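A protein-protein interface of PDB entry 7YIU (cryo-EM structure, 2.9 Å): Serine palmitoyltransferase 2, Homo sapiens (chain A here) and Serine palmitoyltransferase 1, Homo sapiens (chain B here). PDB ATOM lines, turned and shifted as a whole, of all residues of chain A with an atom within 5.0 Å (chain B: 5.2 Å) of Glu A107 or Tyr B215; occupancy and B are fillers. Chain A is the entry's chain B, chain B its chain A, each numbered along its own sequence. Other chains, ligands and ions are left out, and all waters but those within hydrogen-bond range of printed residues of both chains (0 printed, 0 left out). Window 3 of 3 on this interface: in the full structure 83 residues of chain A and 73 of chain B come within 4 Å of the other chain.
Glu A107 touches just one residue of chain B: Tyr B215.
Tyr B215 touches three residues of chain A.
Of the printed residues of chain B, Arg A105 touches Tyr B215 (2.6 Å), Asp B248 (3.5 Å) and Asp B249 (3.9 Å).
Of the printed residues of chain B, Phe A111 touches Lys B214 (3.96 Å), Tyr B215 (3.8 Å) and Lys B218 (3.6 Å).
Printed residues of chain B within 4 Å of Gln A108: Lys B214.
Glu A106 touches none of the printed residues of chain B.
The nearest residue of chain A that does not touch Tyr B215 is Gln A108 (4.3 Å).
The nearest printed residue of chain B that does not touch Arg A105 is Lys B214 (4.9 Å).
Among the printed residues, merely in contact across the chains: Arg A105 with Asp B248, Glu A107 with Tyr B215, Gln A108 with Lys B214, Phe A111 with Lys B214, Phe A111 with Tyr B215 and Phe A111 with Lys B218.
Of the 10 printed residues of chain B, 5 touch a printed residue of chain A.
Of the 6 printed residues of chain A, 4 touch a printed residue of chain B.
Printed residues of chain A that touch a printed residue of chain B: Arg A105, Glu A107, Gln A108 and Phe A111.
The guanidinium group (NH1) of Arg A105 lies within salt-bridge range of the side-chain carboxylate (OD1) of Asp B249.
The guanidinium group (NH1) of Arg A105 lies within hydrogen-bond range of the side-chain hydroxyl (OH) of Tyr B215, 2.6 Å away.
OD1 of Asp B249 lies within hydrogen-bond range of OH of Tyr B215, 2.5 Å away.
The guanidinium group (NH1) of Arg A105 is in hydrogen-bond range of the side-chain amide oxygen (OE1) of Gln A108 (3.3 Å).
OE1 of Glu A107 is in salt-bridge range of NH2 of Arg A105 (3.6 Å).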
ATOM      1  N   ARG A 105     -16.108 -17.344 -17.441  1.00  0.00           N
ATOM      2  CA  ARG A 105     -15.946 -16.795 -16.107  1.00  0.00           C
ATOM      3  C   ARG A 105     -15.527 -15.340 -16.228  1.00  0.00           C
ATOM      4  O   ARG A 105     -15.005 -14.919 -17.257  1.00  0.00           O
ATOM      5  CB  ARG A 105     -14.876 -17.553 -15.329  1.00  0.00           C
ATOM      6  CG  ARG A 105     -14.972 -19.061 -15.402  1.00  0.00           C
ATOM      7  CD  ARG A 105     -13.707 -19.705 -14.865  1.00  0.00           C
ATOM      8  NE  ARG A 105     -13.448 -19.336 -13.479  1.00  0.00           N
ATOM      9  CZ  ARG A 105     -12.237 -19.136 -12.971  1.00  0.00           C
ATOM     10  NH1 ARG A 105     -11.165 -19.266 -13.734  1.00  0.00           N
ATOM     11  NH2 ARG A 105     -12.096 -18.804 -11.698  1.00  0.00           N
ATOM     12  N   GLU A 106     -15.719 -14.572 -15.162  1.00  0.00           N
ATOM     13  CA  GLU A 106     -15.355 -13.162 -15.177  1.00  0.00           C
ATOM     14  C   GLU A 106     -13.846 -12.952 -15.242  1.00  0.00           C
ATOM     15  O   GLU A 106     -13.377 -11.970 -15.812  1.00  0.00           O
ATOM     16  CB  GLU A 106     -15.928 -12.446 -13.958  1.00  0.00           C
ATOM     17  CG  GLU A 106     -16.521 -11.084 -14.269  1.00  0.00           C
ATOM     18  CD  GLU A 106     -17.410 -10.572 -13.156  1.00  0.00           C
ATOM     19  OE1 GLU A 106     -17.353 -11.143 -12.048  1.00  0.00           O
ATOM     20  OE2 GLU A 106     -18.161  -9.602 -13.386  1.00  0.00           O
ATOM     21  N   GLU A 107     -13.083 -13.882 -14.675  1.00  0.00           N
ATOM     22  CA  GLU A 107     -11.631 -13.790 -14.670  1.00  0.00           C
ATOM     23  C   GLU A 107     -10.970 -14.539 -15.823  1.00  0.00           C
ATOM     24  O   GLU A 107      -9.845 -15.002 -15.694  1.00  0.00           O
ATOM     25  CB  GLU A 107     -11.078 -14.311 -13.346  1.00  0.00           C
ATOM     26  CG  GLU A 107     -11.890 -15.439 -12.738  1.00  0.00           C
ATOM     27  CD  GLU A 107     -12.945 -14.941 -11.772  1.00  0.00           C
ATOM     28  OE1 GLU A 107     -13.855 -15.723 -11.423  1.00  0.00           O
ATOM     29  OE2 GLU A 107     -12.865 -13.764 -11.365  1.00  0.00           O
ATOM     30  N   GLN A 108     -11.669 -14.643 -16.947  1.00  0.00           N
ATOM     31  CA  GLN A 108     -11.161 -15.329 -18.124  1.00  0.00           C
ATOM     32  C   GLN A 108     -11.713 -14.677 -19.377  1.00  0.00           C
ATOM     33  O   GLN A 108     -11.907 -15.338 -20.392  1.00  0.00           O
ATOM     34  CB  GLN A 108     -11.589 -16.788 -18.105  1.00  0.00           C
ATOM     35  CG  GLN A 108     -10.743 -17.685 -17.229  1.00  0.00           C
ATOM     36  CD  GLN A 108     -10.821 -19.125 -17.668  1.00  0.00           C
ATOM     37  OE1 GLN A 108     -10.665 -20.038 -16.868  1.00  0.00           O
ATOM     38  NE2 GLN A 108     -11.071 -19.336 -18.948  1.00  0.00           N
ATOM     39  N   LYS A 109     -11.963 -13.376 -19.310  1.00  0.00           N
ATOM     40  CA  LYS A 109     -12.507 -12.644 -20.445  1.00  0.00           C
ATOM     41  C   LYS A 109     -11.428 -12.162 -21.407  1.00  0.00           C
ATOM     42  O   LYS A 109     -11.734 -11.628 -22.468  1.00  0.00           O
ATOM     43  CB  LYS A 109     -13.330 -11.455 -19.957  1.00  0.00           C
ATOM     44  CG  LYS A 109     -14.719 -11.823 -19.470  1.00  0.00           C
ATOM     45  CD  LYS A 109     -15.573 -10.583 -19.259  1.00  0.00           C
ATOM     46  CE  LYS A 109     -16.972 -10.773 -19.823  1.00  0.00           C
ATOM     47  NZ  LYS A 109     -17.147 -10.081 -21.130  1.00  0.00           N
ATOM     48  N   PHE A 111      -8.909 -14.301 -22.375  1.00  0.00           N
ATOM     49  CA  PHE A 111      -8.475 -15.457 -23.137  1.00  0.00           C
ATOM     50  C   PHE A 111      -9.216 -15.485 -24.462  1.00  0.00           C
ATOM     51  O   PHE A 111     -10.334 -14.997 -24.561  1.00  0.00           O
ATOM     52  CB  PHE A 111      -8.786 -16.752 -22.390  1.00  0.00           C
ATOM     53  CG  PHE A 111      -8.056 -16.909 -21.091  1.00  0.00           C
ATOM     54  CD1 PHE A 111      -7.863 -15.834 -20.249  1.00  0.00           C
ATOM     55  CD2 PHE A 111      -7.586 -18.146 -20.703  1.00  0.00           C
ATOM     56  CE1 PHE A 111      -7.202 -15.987 -19.050  1.00  0.00           C
ATOM     57  CE2 PHE A 111      -6.926 -18.306 -19.506  1.00  0.00           C
ATOM     58  CZ  PHE A 111      -6.734 -17.224 -18.678  1.00  0.00           C
ATOM     59  N   VAL B 211      -0.642 -23.393 -12.349  1.00  0.00           N
ATOM     60  CA  VAL B 211      -1.870 -22.609 -12.382  1.00  0.00           C
ATOM     61  C   VAL B 211      -1.548 -21.128 -12.489  1.00  0.00           C
ATOM     62  O   VAL B 211      -2.365 -20.342 -12.951  1.00  0.00           O
ATOM     63  CB  VAL B 211      -2.739 -22.848 -11.134  1.00  0.00           C
ATOM     64  CG1 VAL B 211      -3.475 -21.579 -10.745  1.00  0.00           C
ATOM     65  CG2 VAL B 211      -3.722 -23.978 -11.378  1.00  0.00           C
ATOM     66  N   LYS B 212      -0.351 -20.752 -12.057  1.00  0.00           N
ATOM     67  CA  LYS B 212       0.079 -19.362 -12.116  1.00  0.00           C
ATOM     68  C   LYS B 212       0.571 -19.015 -13.509  1.00  0.00           C
ATOM     69  O   LYS B 212       0.608 -17.854 -13.886  1.00  0.00           O
ATOM     70  CB  LYS B 212       1.183 -19.098 -11.096  1.00  0.00           C
ATOM     71  CG  LYS B 212       0.691 -19.016  -9.663  1.00  0.00           C
ATOM     72  CD  LYS B 212       1.806 -18.593  -8.723  1.00  0.00           C
ATOM     73  CE  LYS B 212       3.154 -19.107  -9.198  1.00  0.00           C
ATOM     74  NZ  LYS B 212       3.748 -20.076  -8.238  1.00  0.00           N
ATOM     75  N   LEU B 213       0.956 -20.030 -14.268  1.00  0.00           N
ATOM     76  CA  LEU B 213       1.441 -19.841 -15.626  1.00  0.00           C
ATOM     77  C   LEU B 213       0.267 -19.747 -16.583  1.00  0.00           C
ATOM     78  O   LEU B 213       0.383 -19.191 -17.665  1.00  0.00           O
ATOM     79  CB  LEU B 213       2.328 -21.013 -16.036  1.00  0.00           C
ATOM     80  CG  LEU B 213       3.803 -20.760 -16.335  1.00  0.00           C
ATOM     81  CD1 LEU B 213       4.384 -19.745 -15.368  1.00  0.00           C
ATOM     82  CD2 LEU B 213       4.577 -22.066 -16.269  1.00  0.00           C
ATOM     83  N   LYS B 214      -0.868 -20.303 -16.179  1.00  0.00           N
ATOM     84  CA  LYS B 214      -2.067 -20.294 -17.007  1.00  0.00           C
ATOM     85  C   LYS B 214      -2.638 -18.895 -17.143  1.00  0.00           C
ATOM     86  O   LYS B 214      -3.002 -18.466 -18.230  1.00  0.00           O
ATOM     87  CB  LYS B 214      -3.123 -21.225 -16.417  1.00  0.00           C
ATOM     88  CG  LYS B 214      -4.513 -21.032 -16.995  1.00  0.00           C
ATOM     89  CD  LYS B 214      -5.580 -21.192 -15.928  1.00  0.00           C
ATOM     90  CE  LYS B 214      -6.954 -21.357 -16.550  1.00  0.00           C
ATOM     91  NZ  LYS B 214      -7.845 -22.201 -15.713  1.00  0.00           N
ATOM     92  N   TYR B 215      -2.707 -18.178 -16.029  1.00  0.00           N
ATOM     93  CA  TYR B 215      -3.244 -16.827 -16.019  1.00  0.00           C
ATOM     94  C   TYR B 215      -2.279 -15.787 -16.574  1.00  0.00           C
ATOM     95  O   TYR B 215      -2.687 -14.693 -16.950  1.00  0.00           O
ATOM     96  CB  TYR B 215      -3.680 -16.446 -14.606  1.00  0.00           C
ATOM     97  CG  TYR B 215      -4.994 -17.072 -14.219  1.00  0.00           C
ATOM     98  CD1 TYR B 215      -6.149 -16.785 -14.926  1.00  0.00           C
ATOM     99  CD2 TYR B 215      -5.078 -17.969 -13.166  1.00  0.00           C
ATOM    100  CE1 TYR B 215      -7.353 -17.363 -14.588  1.00  0.00           C
ATOM    101  CE2 TYR B 215      -6.278 -18.551 -12.822  1.00  0.00           C
ATOM    102  CZ  TYR B 215      -7.410 -18.242 -13.537  1.00  0.00           C
ATOM    103  OH  TYR B 215      -8.610 -18.816 -13.203  1.00  0.00           O
ATOM    104  N   LYS B 216      -1.001 -16.136 -16.638  1.00  0.00           N
ATOM    105  CA  LYS B 216       0.018 -15.229 -17.138  1.00  0.00           C
ATOM    106  C   LYS B 216       0.236 -15.326 -18.643  1.00  0.00           C
ATOM    107  O   LYS B 216       0.715 -14.380 -19.255  1.00  0.00           O
ATOM    108  CB  LYS B 216       1.336 -15.472 -16.408  1.00  0.00           C
ATOM    109  CG  LYS B 216       2.372 -14.389 -16.630  1.00  0.00           C
ATOM    110  CD  LYS B 216       3.773 -14.969 -16.608  1.00  0.00           C
ATOM    111  CE  LYS B 216       4.223 -15.254 -15.189  1.00  0.00           C
ATOM    112  NZ  LYS B 216       5.581 -14.703 -14.925  1.00  0.00           N
ATOM    113  N   TYR B 217      -0.111 -16.461 -19.238  1.00  0.00           N
ATOM    114  CA  TYR B 217       0.076 -16.652 -20.674  1.00  0.00           C
ATOM    115  C   TYR B 217      -1.214 -16.977 -21.421  1.00  0.00           C
ATOM    116  O   TYR B 217      -1.183 -17.321 -22.596  1.00  0.00           O
ATOM    117  CB  TYR B 217       1.134 -17.718 -20.948  1.00  0.00           C
ATOM    118  CG  TYR B 217       2.528 -17.292 -20.556  1.00  0.00           C
ATOM    119  CD1 TYR B 217       3.281 -16.471 -21.377  1.00  0.00           C
ATOM    120  CD2 TYR B 217       3.086 -17.708 -19.363  1.00  0.00           C
ATOM    121  CE1 TYR B 217       4.551 -16.077 -21.017  1.00  0.00           C
ATOM    122  CE2 TYR B 217       4.353 -17.318 -18.996  1.00  0.00           C
ATOM    123  CZ  TYR B 217       5.078 -16.503 -19.827  1.00  0.00           C
ATOM    124  OH  TYR B 217       6.340 -16.116 -19.457  1.00  0.00           O
ATOM    125  N   LYS B 218      -2.341 -16.870 -20.726  1.00  0.00           N
ATOM    126  CA  LYS B 218      -3.663 -17.109 -21.308  1.00  0.00           C
ATOM    127  C   LYS B 218      -3.878 -18.444 -22.031  1.00  0.00           C
ATOM    128  O   LYS B 218      -4.328 -18.483 -23.169  1.00  0.00           O
ATOM    129  CB  LYS B 218      -4.064 -15.940 -22.207  1.00  0.00           C
ATOM    130  CG  LYS B 218      -4.686 -14.783 -21.450  1.00  0.00           C
ATOM    131  CD  LYS B 218      -3.802 -13.557 -21.520  1.00  0.00           C
ATOM    132  CE  LYS B 218      -3.712 -12.867 -20.174  1.00  0.00           C
ATOM    133  NZ  LYS B 218      -3.152 -11.495 -20.301  1.00  0.00           N
ATOM    134  N   ASP B 248     -12.393 -24.559  -9.759  1.00  0.00           N
ATOM    135  CA  ASP B 248     -12.836 -23.774 -10.903  1.00  0.00           C
ATOM    136  C   ASP B 248     -11.696 -23.293 -11.786  1.00  0.00           C
ATOM    137  O   ASP B 248     -11.955 -22.638 -12.798  1.00  0.00           O
ATOM    138  CB  ASP B 248     -13.646 -22.566 -10.435  1.00  0.00           C
ATOM    139  CG  ASP B 248     -14.981 -22.952  -9.853  1.00  0.00           C
ATOM    140  OD1 ASP B 248     -15.521 -24.003 -10.247  1.00  0.00           O
ATOM    141  OD2 ASP B 248     -15.498 -22.199  -9.002  1.00  0.00           O
ATOM    142  N   ASP B 249     -10.452 -23.600 -11.436  1.00  0.00           N
ATOM    143  CA  ASP B 249      -9.292 -23.104 -12.162  1.00  0.00           C
ATOM    144  C   ASP B 249      -8.793 -24.058 -13.235  1.00  0.00           C
ATOM    145  O   ASP B 249      -7.803 -23.746 -13.898  1.00  0.00           O
ATOM    146  CB  ASP B 249      -8.152 -22.817 -11.184  1.00  0.00           C
ATOM    147  CG  ASP B 249      -8.209 -21.426 -10.614  1.00  0.00           C
ATOM    148  OD1 ASP B 249      -8.268 -20.465 -11.403  1.00  0.00           O
ATOM    149  OD2 ASP B 249      -8.192 -21.286  -9.377  1.00  0.00           O
